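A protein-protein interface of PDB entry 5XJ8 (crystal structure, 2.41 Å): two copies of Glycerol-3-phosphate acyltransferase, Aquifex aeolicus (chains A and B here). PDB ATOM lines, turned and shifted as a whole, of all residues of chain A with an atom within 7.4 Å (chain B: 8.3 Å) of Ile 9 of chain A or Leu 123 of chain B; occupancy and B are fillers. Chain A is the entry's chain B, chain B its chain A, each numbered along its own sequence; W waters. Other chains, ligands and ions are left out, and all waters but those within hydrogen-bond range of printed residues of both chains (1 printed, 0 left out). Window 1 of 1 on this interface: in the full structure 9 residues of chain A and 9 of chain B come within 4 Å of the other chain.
The side-chain hydroxyl (OG) of Ser 118 of chain B is in hydrogen-bond range of the side-chain hydroxyl (OG) of Ser 120 of chain B (3.0 Å).
The backbone carbonyl oxygen (O) of Tyr 12 of chain A is in hydrogen-bond range of the side-chain hydroxyl (OG) of Ser 16 of chain A (2.9 Å).
The backbone NH (N) of Val 97 of chain A sits at hydrogen-bond distance from the side-chain hydroxyl (OG) of Ser 16 of chain A.
Among the printed residues, pairs that only touch across the chains: Ile 9 of chain A with Phe 126 of chain B (3.4 Å), Phe 6 of chain A with Leu 127 of chain B (3.4 Å), Val 97 of chain A with Ser 120 of chain B (3.5 Å), Gly 2 of chain A with Leu 130 of chain B (3.5 Å), Leu 5 of chain A with Phe 126 of chain B (3.6 Å), Val 97 of chain A with Pro 119 of chain B (3.6 Å), Leu 13 of chain A with Leu 127 of chain B (3.6 Å), Phe 6 of chain A with Leu 130 of chain B (3.7 Å), Tyr 12 of chain A with Leu 123 of chain B (3.8 Å), Ile 9 of chain A with Leu 127 of chain B (3.8 Å), Leu 13 of chain A with Leu 123 of chain B (3.96 Å), Val 97 of chain A with Leu 123 of chain B (3.97 Å) and Ile 9 of chain A with Leu 123 of chain B (3.99 Å).
Printed residues of chain B within 4 Å of Gly 2 of chain A: Leu 130.
Of the printed residues of chain B, Ile 9 of chain A touches Leu 123 (3.99 Å), Phe 126 (3.4 Å) and Leu 127 (3.8 Å).
Of the printed residues of chain B, Leu 13 of chain A touches Leu 123 and Leu 127.
Printed residues of chain A within 4 Å of Pro 119 of chain B: Val 97 (3.6 Å).
No residue of chain A comes within 4 Å of Ala 122 of chain B.
Of the printed residues of chain A, Leu 123 of chain B touches Ile 9 (3.99 Å), Tyr 12 (3.8 Å), Leu 13 (3.96 Å) and Val 97 (3.97 Å).
Of the 20 printed residues of chain A, 7 touch a printed residue of chain B.
Hydrophobic or aromatic side chains of chain A that line the printed part of chain B: Leu 5, Phe 6, Ile 9, Tyr 12, Leu 13 and Val 97.
Among the printed residues, no Asp or Glu carboxylate lies within 4 Å of a Lys or Arg side-chain nitrogen of the other chain.
No position is printed for both chains.
Of the 13 pairs that touch across the chains among the printed residues, none has its exchanged pair printed and touching as well.
Water W1 bridges OG of Ser 120 of chain B (2.7 Å) and O of Val 97 of chain A (3.2 Å).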
ATOM      1  N   GLY A   2      22.379 -12.528   9.339  1.00  0.00           N
ATOM      2  CA  GLY A   2      23.044 -13.520  10.166  1.00  0.00           C
ATOM      3  C   GLY A   2      22.270 -13.847  11.428  1.00  0.00           C
ATOM      4  O   GLY A   2      21.693 -14.928  11.553  1.00  0.00           O
ATOM      5  N   SER A   3      22.263 -12.904  12.372  1.00  0.00           N
ATOM      6  CA  SER A   3      21.482 -13.087  13.591  1.00  0.00           C
ATOM      7  C   SER A   3      19.991 -13.139  13.284  1.00  0.00           C
ATOM      8  O   SER A   3      19.241 -13.887  13.923  1.00  0.00           O
ATOM      9  CB  SER A   3      21.786 -11.963  14.582  1.00  0.00           C
ATOM     10  OG  SER A   3      23.028 -12.170  15.232  1.00  0.00           O
ATOM     11  N   ALA A   4      19.544 -12.350  12.304  1.00  0.00           N
ATOM     12  CA  ALA A   4      18.134 -12.346  11.930  1.00  0.00           C
ATOM     13  C   ALA A   4      17.719 -13.686  11.339  1.00  0.00           C
ATOM     14  O   ALA A   4      16.654 -14.221  11.671  1.00  0.00           O
ATOM     15  CB  ALA A   4      17.867 -11.216  10.936  1.00  0.00           C
ATOM     16  N   LEU A   5      18.548 -14.237  10.449  1.00  0.00           N
ATOM     17  CA  LEU A   5      18.261 -15.544   9.867  1.00  0.00           C
ATOM     18  C   LEU A   5      18.123 -16.608  10.948  1.00  0.00           C
ATOM     19  O   LEU A   5      17.245 -17.475  10.868  1.00  0.00           O
ATOM     20  CB  LEU A   5      19.360 -15.920   8.874  1.00  0.00           C
ATOM     21  CG  LEU A   5      19.076 -17.079   7.919  1.00  0.00           C
ATOM     22  CD1 LEU A   5      17.783 -16.846   7.154  1.00  0.00           C
ATOM     23  CD2 LEU A   5      20.244 -17.270   6.966  1.00  0.00           C
ATOM     24  N   PHE A   6      18.983 -16.553  11.968  1.00  0.00           N
ATOM     25  CA  PHE A   6      18.866 -17.467  13.100  1.00  0.00           C
ATOM     26  C   PHE A   6      17.497 -17.349  13.757  1.00  0.00           C
ATOM     27  O   PHE A   6      16.829 -18.355  14.022  1.00  0.00           O
ATOM     28  CB  PHE A   6      19.980 -17.178  14.111  1.00  0.00           C
ATOM     29  CG  PHE A   6      19.941 -18.049  15.338  1.00  0.00           C
ATOM     30  CD1 PHE A   6      19.143 -17.717  16.424  1.00  0.00           C
ATOM     31  CD2 PHE A   6      20.720 -19.192  15.414  1.00  0.00           C
ATOM     32  CE1 PHE A   6      19.109 -18.516  17.551  1.00  0.00           C
ATOM     33  CE2 PHE A   6      20.693 -19.994  16.540  1.00  0.00           C
ATOM     34  CZ  PHE A   6      19.886 -19.656  17.609  1.00  0.00           C
ATOM     35  N   LEU A   7      17.062 -16.116  14.025  1.00  0.00           N
ATOM     36  CA  LEU A   7      15.792 -15.903  14.711  1.00  0.00           C
ATOM     37  C   LEU A   7      14.613 -16.335  13.849  1.00  0.00           C
ATOM     38  O   LEU A   7      13.659 -16.938  14.354  1.00  0.00           O
ATOM     39  CB  LEU A   7      15.665 -14.435  15.108  1.00  0.00           C
ATOM     40  CG  LEU A   7      14.342 -13.934  15.686  1.00  0.00           C
ATOM     41  CD1 LEU A   7      13.898 -14.775  16.874  1.00  0.00           C
ATOM     42  CD2 LEU A   7      14.497 -12.484  16.085  1.00  0.00           C
ATOM     43  N   VAL A   8      14.659 -16.041  12.547  1.00  0.00           N
ATOM     44  CA  VAL A   8      13.550 -16.395  11.664  1.00  0.00           C
ATOM     45  C   VAL A   8      13.403 -17.909  11.569  1.00  0.00           C
ATOM     46  O   VAL A   8      12.290 -18.445  11.628  1.00  0.00           O
ATOM     47  CB  VAL A   8      13.743 -15.752  10.278  1.00  0.00           C
ATOM     48  CG1 VAL A   8      12.779 -16.355   9.268  1.00  0.00           C
ATOM     49  CG2 VAL A   8      13.552 -14.245  10.365  1.00  0.00           C
ATOM     50  N   ILE A   9      14.521 -18.622  11.426  1.00  0.00           N
ATOM     51  CA  ILE A   9      14.463 -20.080  11.377  1.00  0.00           C
ATOM     52  C   ILE A   9      14.012 -20.642  12.718  1.00  0.00           C
ATOM     53  O   ILE A   9      13.210 -21.583  12.774  1.00  0.00           O
ATOM     54  CB  ILE A   9      15.825 -20.650  10.947  1.00  0.00           C
ATOM     55  CG1 ILE A   9      16.109 -20.282   9.492  1.00  0.00           C
ATOM     56  CG2 ILE A   9      15.860 -22.160  11.131  1.00  0.00           C
ATOM     57  CD1 ILE A   9      17.573 -20.218   9.165  1.00  0.00           C
ATOM     58  N   PHE A  10      14.511 -20.073  13.819  1.00  0.00           N
ATOM     59  CA  PHE A  10      14.065 -20.507  15.139  1.00  0.00           C
ATOM     60  C   PHE A  10      12.566 -20.298  15.306  1.00  0.00           C
ATOM     61  O   PHE A  10      11.870 -21.158  15.857  1.00  0.00           O
ATOM     62  CB  PHE A  10      14.833 -19.762  16.230  1.00  0.00           C
ATOM     63  CG  PHE A  10      14.193 -19.852  17.586  1.00  0.00           C
ATOM     64  CD1 PHE A  10      14.246 -21.028  18.314  1.00  0.00           C
ATOM     65  CD2 PHE A  10      13.532 -18.762  18.130  1.00  0.00           C
ATOM     66  CE1 PHE A  10      13.657 -21.117  19.560  1.00  0.00           C
ATOM     67  CE2 PHE A  10      12.940 -18.843  19.376  1.00  0.00           C
ATOM     68  CZ  PHE A  10      13.002 -20.023  20.093  1.00  0.00           C
ATOM     69  N   ALA A  11      12.050 -19.161  14.831  1.00  0.00           N
ATOM     70  CA  ALA A  11      10.614 -18.916  14.891  1.00  0.00           C
ATOM     71  C   ALA A  11       9.838 -19.930  14.063  1.00  0.00           C
ATOM     72  O   ALA A  11       8.722 -20.311  14.434  1.00  0.00           O
ATOM     73  CB  ALA A  11      10.301 -17.498  14.413  1.00  0.00           C
ATOM     74  N   TYR A  12      10.408 -20.376  12.941  1.00  0.00           N
ATOM     75  CA  TYR A  12       9.718 -21.356  12.109  1.00  0.00           C
ATOM     76  C   TYR A  12       9.759 -22.742  12.741  1.00  0.00           C
ATOM     77  O   TYR A  12       8.759 -23.469  12.719  1.00  0.00           O
ATOM     78  CB  TYR A  12      10.334 -21.387  10.712  1.00  0.00           C
ATOM     79  CG  TYR A  12       9.750 -22.466   9.832  1.00  0.00           C
ATOM     80  CD1 TYR A  12       8.450 -22.369   9.355  1.00  0.00           C
ATOM     81  CD2 TYR A  12      10.495 -23.587   9.486  1.00  0.00           C
ATOM     82  CE1 TYR A  12       7.908 -23.354   8.553  1.00  0.00           C
ATOM     83  CE2 TYR A  12       9.961 -24.579   8.684  1.00  0.00           C
ATOM     84  CZ  TYR A  12       8.667 -24.457   8.221  1.00  0.00           C
ATOM     85  OH  TYR A  12       8.128 -25.439   7.422  1.00  0.00           O
ATOM     86  N   LEU A  13      10.906 -23.126  13.308  1.00  0.00           N
ATOM     87  CA  LEU A  13      10.999 -24.422  13.970  1.00  0.00           C
ATOM     88  C   LEU A  13      10.156 -24.457  15.238  1.00  0.00           C
ATOM     89  O   LEU A  13       9.456 -25.445  15.497  1.00  0.00           O
ATOM     90  CB  LEU A  13      12.460 -24.745  14.282  1.00  0.00           C
ATOM     91  CG  LEU A  13      13.351 -24.948  13.057  1.00  0.00           C
ATOM     92  CD1 LEU A  13      14.814 -24.930  13.454  1.00  0.00           C
ATOM     93  CD2 LEU A  13      13.000 -26.249  12.350  1.00  0.00           C
ATOM     94  N   LEU A  14      10.205 -23.390  16.040  1.00  0.00           N
ATOM     95  CA  LEU A  14       9.370 -23.329  17.235  1.00  0.00           C
ATOM     96  C   LEU A  14       7.892 -23.320  16.872  1.00  0.00           C
ATOM     97  O   LEU A  14       7.081 -23.991  17.521  1.00  0.00           O
ATOM     98  CB  LEU A  14       9.723 -22.094  18.063  1.00  0.00           C
ATOM     99  CG  LEU A  14       8.952 -21.956  19.376  1.00  0.00           C
ATOM    100  CD1 LEU A  14       9.269 -23.121  20.300  1.00  0.00           C
ATOM    101  CD2 LEU A  14       9.260 -20.630  20.049  1.00  0.00           C
ATOM    102  N   GLY A  15       7.523 -22.563  15.838  1.00  0.00           N
ATOM    103  CA  GLY A  15       6.147 -22.561  15.379  1.00  0.00           C
ATOM    104  C   GLY A  15       5.694 -23.890  14.816  1.00  0.00           C
ATOM    105  O   GLY A  15       4.492 -24.174  14.807  1.00  0.00           O
ATOM    106  N   SER A  16       6.633 -24.720  14.356  1.00  0.00           N
ATOM    107  CA  SER A  16       6.301 -26.020  13.787  1.00  0.00           C
ATOM    108  C   SER A  16       5.882 -27.045  14.834  1.00  0.00           C
ATOM    109  O   SER A  16       5.494 -28.157  14.459  1.00  0.00           O
ATOM    110  CB  SER A  16       7.488 -26.557  12.984  1.00  0.00           C
ATOM    111  OG  SER A  16       7.548 -25.957  11.703  1.00  0.00           O
ATOM    112  N   PHE A  84       9.369 -10.817   9.291  1.00  0.00           N
ATOM    113  CA  PHE A  84       9.595 -12.190   8.862  1.00  0.00           C
ATOM    114  C   PHE A  84       9.697 -13.163  10.027  1.00  0.00           C
ATOM    115  O   PHE A  84       9.473 -14.363   9.832  1.00  0.00           O
ATOM    116  CB  PHE A  84      10.850 -12.256   7.992  1.00  0.00           C
ATOM    117  CG  PHE A  84      10.710 -11.517   6.692  1.00  0.00           C
ATOM    118  CD1 PHE A  84       9.742 -11.890   5.774  1.00  0.00           C
ATOM    119  CD2 PHE A  84      11.526 -10.439   6.397  1.00  0.00           C
ATOM    120  CE1 PHE A  84       9.599 -11.211   4.580  1.00  0.00           C
ATOM    121  CE2 PHE A  84      11.388  -9.753   5.204  1.00  0.00           C
ATOM    122  CZ  PHE A  84      10.422 -10.140   4.295  1.00  0.00           C
ATOM    123  N   THR A  85      10.022 -12.683  11.230  1.00  0.00           N
ATOM    124  CA  THR A  85       9.969 -13.548  12.404  1.00  0.00           C
ATOM    125  C   THR A  85       8.530 -13.937  12.724  1.00  0.00           C
ATOM    126  O   THR A  85       8.218 -15.122  12.891  1.00  0.00           O
ATOM    127  CB  THR A  85      10.617 -12.859  13.605  1.00  0.00           C
ATOM    128  OG1 THR A  85      12.016 -12.670  13.357  1.00  0.00           O
ATOM    129  CG2 THR A  85      10.437 -13.700  14.861  1.00  0.00           C
ATOM    130  N   ALA A  88       7.268 -16.251  10.225  1.00  0.00           N
ATOM    131  CA  ALA A  88       7.850 -17.582  10.365  1.00  0.00           C
ATOM    132  C   ALA A  88       7.130 -18.396  11.431  1.00  0.00           C
ATOM    133  O   ALA A  88       6.915 -19.602  11.262  1.00  0.00           O
ATOM    134  CB  ALA A  88       9.338 -17.471  10.692  1.00  0.00           C
ATOM    135  N   VAL A  97       7.240 -28.238   9.862  1.00  0.00           N
ATOM    136  CA  VAL A  97       8.292 -29.045   9.259  1.00  0.00           C
ATOM    137  C   VAL A  97       8.355 -30.439   9.870  1.00  0.00           C
ATOM    138  O   VAL A  97       8.900 -31.361   9.254  1.00  0.00           O
ATOM    139  CB  VAL A  97       9.645 -28.309   9.388  1.00  0.00           C
ATOM    140  CG1 VAL A  97      10.160 -28.371  10.821  1.00  0.00           C
ATOM    141  CG2 VAL A  97      10.662 -28.877   8.414  1.00  0.00           C
ATOM    142  N   PHE A 101       4.188 -30.836   7.144  1.00  0.00           N
ATOM    143  CA  PHE A 101       3.639 -29.549   6.708  1.00  0.00           C
ATOM    144  C   PHE A 101       2.111 -29.556   6.717  1.00  0.00           C
ATOM    145  O   PHE A 101       1.464 -28.959   5.855  1.00  0.00           O
ATOM    146  CB  PHE A 101       4.175 -29.152   5.328  1.00  0.00           C
ATOM    147  CG  PHE A 101       5.677 -29.181   5.227  1.00  0.00           C
ATOM    148  CD1 PHE A 101       6.343 -30.339   4.858  1.00  0.00           C
ATOM    149  CD2 PHE A 101       6.422 -28.046   5.500  1.00  0.00           C
ATOM    150  CE1 PHE A 101       7.721 -30.364   4.766  1.00  0.00           C
ATOM    151  CE2 PHE A 101       7.801 -28.067   5.408  1.00  0.00           C
ATOM    152  CZ  PHE A 101       8.450 -29.226   5.042  1.00  0.00           C
ATOM    153  N   PHE B  61      23.650 -26.106  -3.262  1.00  0.00           N
ATOM    154  CA  PHE B  61      22.598 -26.754  -2.488  1.00  0.00           C
ATOM    155  C   PHE B  61      21.698 -27.593  -3.385  1.00  0.00           C
ATOM    156  O   PHE B  61      21.303 -28.706  -3.018  1.00  0.00           O
ATOM    157  CB  PHE B  61      21.789 -25.690  -1.739  1.00  0.00           C
ATOM    158  CG  PHE B  61      20.548 -26.210  -1.056  1.00  0.00           C
ATOM    159  CD1 PHE B  61      19.347 -26.323  -1.746  1.00  0.00           C
ATOM    160  CD2 PHE B  61      20.574 -26.546   0.287  1.00  0.00           C
ATOM    161  CE1 PHE B  61      18.207 -26.788  -1.115  1.00  0.00           C
ATOM    162  CE2 PHE B  61      19.435 -27.008   0.925  1.00  0.00           C
ATOM    163  CZ  PHE B  61      18.251 -27.129   0.223  1.00  0.00           C
ATOM    164  N   LEU B 111      24.046 -30.191   2.705  1.00  0.00           N
ATOM    165  CA  LEU B 111      22.816 -29.632   3.258  1.00  0.00           C
ATOM    166  C   LEU B 111      21.639 -29.887   2.328  1.00  0.00           C
ATOM    167  O   LEU B 111      20.526 -30.169   2.785  1.00  0.00           O
ATOM    168  CB  LEU B 111      22.975 -28.134   3.513  1.00  0.00           C
ATOM    169  CG  LEU B 111      21.712 -27.438   4.027  1.00  0.00           C
ATOM    170  CD1 LEU B 111      21.350 -27.942   5.416  1.00  0.00           C
ATOM    171  CD2 LEU B 111      21.879 -25.925   4.025  1.00  0.00           C
ATOM    172  N   VAL B 114      20.472 -33.548   2.961  1.00  0.00           N
ATOM    173  CA  VAL B 114      19.709 -33.784   4.182  1.00  0.00           C
ATOM    174  C   VAL B 114      18.364 -33.070   4.132  1.00  0.00           C
ATOM    175  O   VAL B 114      17.400 -33.506   4.772  1.00  0.00           O
ATOM    176  CB  VAL B 114      20.532 -33.372   5.420  1.00  0.00           C
ATOM    177  CG1 VAL B 114      20.671 -31.861   5.504  1.00  0.00           C
ATOM    178  CG2 VAL B 114      19.906 -33.929   6.693  1.00  0.00           C
ATOM    179  N   PHE B 115      18.262 -31.979   3.365  1.00  0.00           N
ATOM    180  CA  PHE B 115      16.989 -31.269   3.269  1.00  0.00           C
ATOM    181  C   PHE B 115      15.957 -32.088   2.504  1.00  0.00           C
ATOM    182  O   PHE B 115      14.772 -32.089   2.859  1.00  0.00           O
ATOM    183  CB  PHE B 115      17.191 -29.905   2.611  1.00  0.00           C
ATOM    184  CG  PHE B 115      15.965 -29.033   2.640  1.00  0.00           C
ATOM    185  CD1 PHE B 115      15.716 -28.203   3.720  1.00  0.00           C
ATOM    186  CD2 PHE B 115      15.060 -29.049   1.590  1.00  0.00           C
ATOM    187  CE1 PHE B 115      14.588 -27.403   3.751  1.00  0.00           C
ATOM    188  CE2 PHE B 115      13.930 -28.253   1.615  1.00  0.00           C
ATOM    189  CZ  PHE B 115      13.695 -27.428   2.696  1.00  0.00           C
ATOM    190  N   SER B 118      15.275 -34.853   5.196  1.00  0.00           N
ATOM    191  CA  SER B 118      14.655 -34.334   6.414  1.00  0.00           C
ATOM    192  C   SER B 118      14.751 -32.815   6.412  1.00  0.00           C
ATOM    193  O   SER B 118      15.800 -32.253   6.766  1.00  0.00           O
ATOM    194  CB  SER B 118      15.319 -34.915   7.658  1.00  0.00           C
ATOM    195  OG  SER B 118      14.779 -34.342   8.835  1.00  0.00           O
ATOM    196  N   PRO B 119      13.684 -32.116   6.018  1.00  0.00           N
ATOM    197  CA  PRO B 119      13.703 -30.650   6.128  1.00  0.00           C
ATOM    198  C   PRO B 119      13.882 -30.163   7.555  1.00  0.00           C
ATOM    199  O   PRO B 119      14.428 -29.073   7.762  1.00  0.00           O
ATOM    200  CB  PRO B 119      12.343 -30.237   5.550  1.00  0.00           C
ATOM    201  CG  PRO B 119      11.937 -31.376   4.676  1.00  0.00           C
ATOM    202  CD  PRO B 119      12.466 -32.607   5.352  1.00  0.00           C
ATOM    203  N   SER B 120      13.451 -30.947   8.547  1.00  0.00           N
ATOM    204  CA  SER B 120      13.586 -30.524   9.938  1.00  0.00           C
ATOM    205  C   SER B 120      15.039 -30.596  10.398  1.00  0.00           C
ATOM    206  O   SER B 120      15.556 -29.646  10.998  1.00  0.00           O
ATOM    207  CB  SER B 120      12.692 -31.380  10.834  1.00  0.00           C
ATOM    208  OG  SER B 120      12.910 -32.759  10.597  1.00  0.00           O
ATOM    209  N   VAL B 121      15.713 -31.716  10.125  1.00  0.00           N
ATOM    210  CA  VAL B 121      17.108 -31.863  10.536  1.00  0.00           C
ATOM    211  C   VAL B 121      17.986 -30.841   9.826  1.00  0.00           C
ATOM    212  O   VAL B 121      18.930 -30.295  10.412  1.00  0.00           O
ATOM    213  CB  VAL B 121      17.587 -33.306  10.281  1.00  0.00           C
ATOM    214  CG1 VAL B 121      19.096 -33.408  10.428  1.00  0.00           C
ATOM    215  CG2 VAL B 121      16.896 -34.267  11.238  1.00  0.00           C
ATOM    216  N   ALA B 122      17.682 -30.555   8.557  1.00  0.00           N
ATOM    217  CA  ALA B 122      18.468 -29.583   7.802  1.00  0.00           C
ATOM    218  C   ALA B 122      18.408 -28.205   8.448  1.00  0.00           C
ATOM    219  O   ALA B 122      19.442 -27.558   8.655  1.00  0.00           O
ATOM    220  CB  ALA B 122      17.973 -29.523   6.357  1.00  0.00           C
ATOM    221  N   LEU B 123      17.199 -27.739   8.775  1.00  0.00           N
ATOM    222  CA  LEU B 123      17.063 -26.421   9.385  1.00  0.00           C
ATOM    223  C   LEU B 123      17.619 -26.405  10.803  1.00  0.00           C
ATOM    224  O   LEU B 123      18.193 -25.399  11.235  1.00  0.00           O
ATOM    225  CB  LEU B 123      15.598 -25.978   9.374  1.00  0.00           C
ATOM    226  CG  LEU B 123      14.944 -25.882   7.994  1.00  0.00           C
ATOM    227  CD1 LEU B 123      13.435 -26.059   8.090  1.00  0.00           C
ATOM    228  CD2 LEU B 123      15.296 -24.564   7.321  1.00  0.00           C
ATOM    229  N   PHE B 124      17.461 -27.505  11.542  1.00  0.00           N
ATOM    230  CA  PHE B 124      18.073 -27.592  12.864  1.00  0.00           C
ATOM    231  C   PHE B 124      19.592 -27.523  12.770  1.00  0.00           C
ATOM    232  O   PHE B 124      20.243 -26.841  13.572  1.00  0.00           O
ATOM    233  CB  PHE B 124      17.641 -28.880  13.566  1.00  0.00           C
ATOM    234  CG  PHE B 124      16.586 -28.678  14.616  1.00  0.00           C
ATOM    235  CD1 PHE B 124      16.872 -27.976  15.776  1.00  0.00           C
ATOM    236  CD2 PHE B 124      15.312 -29.193  14.448  1.00  0.00           C
ATOM    237  CE1 PHE B 124      15.905 -27.788  16.746  1.00  0.00           C
ATOM    238  CE2 PHE B 124      14.339 -29.009  15.417  1.00  0.00           C
ATOM    239  CZ  PHE B 124      14.637 -28.304  16.567  1.00  0.00           C
ATOM    240  N   SER B 125      20.175 -28.224  11.796  1.00  0.00           N
ATOM    241  CA  SER B 125      21.619 -28.161  11.603  1.00  0.00           C
ATOM    242  C   SER B 125      22.059 -26.780  11.139  1.00  0.00           C
ATOM    243  O   SER B 125      23.158 -26.333  11.486  1.00  0.00           O
ATOM    244  CB  SER B 125      22.061 -29.225  10.600  1.00  0.00           C
ATOM    245  OG  SER B 125      21.604 -30.504  10.995  1.00  0.00           O
ATOM    246  N   PHE B 126      21.223 -26.094  10.356  1.00  0.00           N
ATOM    247  CA  PHE B 126      21.546 -24.725   9.970  1.00  0.00           C
ATOM    248  C   PHE B 126      21.488 -23.783  11.166  1.00  0.00           C
ATOM    249  O   PHE B 126      22.253 -22.813  11.225  1.00  0.00           O
ATOM    250  CB  PHE B 126      20.604 -24.250   8.867  1.00  0.00           C
ATOM    251  CG  PHE B 126      21.082 -23.020   8.154  1.00  0.00           C
ATOM    252  CD1 PHE B 126      22.359 -22.961   7.623  1.00  0.00           C
ATOM    253  CD2 PHE B 126      20.258 -21.920   8.019  1.00  0.00           C
ATOM    254  CE1 PHE B 126      22.800 -21.829   6.970  1.00  0.00           C
ATOM    255  CE2 PHE B 126      20.693 -20.785   7.367  1.00  0.00           C
ATOM    256  CZ  PHE B 126      21.966 -20.739   6.841  1.00  0.00           C
ATOM    257  N   LEU B 127      20.591 -24.048  12.122  1.00  0.00           N
ATOM    258  CA  LEU B 127      20.589 -23.284  13.365  1.00  0.00           C
ATOM    259  C   LEU B 127      21.889 -23.487  14.132  1.00  0.00           C
ATOM    260  O   LEU B 127      22.458 -22.530  14.671  1.00  0.00           O
ATOM    261  CB  LEU B 127      19.397 -23.685  14.235  1.00  0.00           C
ATOM    262  CG  LEU B 127      18.108 -22.867  14.148  1.00  0.00           C
ATOM    263  CD1 LEU B 127      17.248 -23.117  15.376  1.00  0.00           C
ATOM    264  CD2 LEU B 127      18.409 -21.388  13.992  1.00  0.00           C
ATOM    265  N   VAL B 128      22.369 -24.732  14.196  1.00  0.00           N
ATOM    266  CA  VAL B 128      23.624 -25.018  14.885  1.00  0.00           C
ATOM    267  C   VAL B 128      24.776 -24.279  14.217  1.00  0.00           C
ATOM    268  O   VAL B 128      25.635 -23.697  14.892  1.00  0.00           O
ATOM    269  CB  VAL B 128      23.872 -26.537  14.927  1.00  0.00           C
ATOM    270  CG1 VAL B 128      25.251 -26.838  15.498  1.00  0.00           C
ATOM    271  CG2 VAL B 128      22.789 -27.230  15.738  1.00  0.00           C
ATOM    272  N   TRP B 129      24.808 -24.281  12.883  1.00  0.00           N
ATOM    273  CA  TRP B 129      25.867 -23.584  12.158  1.00  0.00           C
ATOM    274  C   TRP B 129      25.841 -22.090  12.454  1.00  0.00           C
ATOM    275  O   TRP B 129      26.882 -21.481  12.727  1.00  0.00           O
ATOM    276  CB  TRP B 129      25.722 -23.837  10.657  1.00  0.00           C
ATOM    277  CG  TRP B 129      26.925 -23.446   9.857  1.00  0.00           C
ATOM    278  CD1 TRP B 129      27.898 -24.277   9.390  1.00  0.00           C
ATOM    279  CD2 TRP B 129      27.280 -22.127   9.419  1.00  0.00           C
ATOM    280  NE1 TRP B 129      28.843 -23.560   8.695  1.00  0.00           N
ATOM    281  CE2 TRP B 129      28.485 -22.237   8.697  1.00  0.00           C
ATOM    282  CE3 TRP B 129      26.698 -20.865   9.568  1.00  0.00           C
ATOM    283  CZ2 TRP B 129      29.118 -21.135   8.127  1.00  0.00           C
ATOM    284  CZ3 TRP B 129      27.330 -19.770   9.004  1.00  0.00           C
ATOM    285  CH2 TRP B 129      28.527 -19.913   8.291  1.00  0.00           C
ATOM    286  N   LEU B 130      24.654 -21.481  12.401  1.00  0.00           N
ATOM    287  CA  LEU B 130      24.541 -20.048  12.650  1.00  0.00           C
ATOM    288  C   LEU B 130      24.991 -19.700  14.063  1.00  0.00           C
ATOM    289  O   LEU B 130      25.733 -18.734  14.270  1.00  0.00           O
ATOM    290  CB  LEU B 130      23.104 -19.588  12.412  1.00  0.00           C
ATOM    291  CG  LEU B 130      22.753 -19.216  10.970  1.00  0.00           C
ATOM    292  CD1 LEU B 130      21.247 -19.194  10.773  1.00  0.00           C
ATOM    293  CD2 LEU B 130      23.366 -17.874  10.605  1.00  0.00           C
ATOM    294  N   PHE B 153      21.079 -35.479  14.943  1.00  0.00           N
ATOM    295  CA  PHE B 153      19.658 -35.202  14.765  1.00  0.00           C
ATOM    296  C   PHE B 153      18.968 -36.330  14.009  1.00  0.00           C
ATOM    297  O   PHE B 153      17.852 -36.728  14.360  1.00  0.00           O
ATOM    298  CB  PHE B 153      19.462 -33.875  14.032  1.00  0.00           C
ATOM    299  CG  PHE B 153      19.944 -32.678  14.801  1.00  0.00           C
ATOM    300  CD1 PHE B 153      20.051 -32.719  16.181  1.00  0.00           C
ATOM    301  CD2 PHE B 153      20.291 -31.512  14.139  1.00  0.00           C
ATOM    302  CE1 PHE B 153      20.495 -31.618  16.887  1.00  0.00           C
ATOM    303  CE2 PHE B 153      20.735 -30.408  14.840  1.00  0.00           C
ATOM    304  CZ  PHE B 153      20.838 -30.461  16.216  1.00  0.00           C
HETATM  305  O   HOH W   1      11.344 -33.347   8.455  1.00  0.00           O
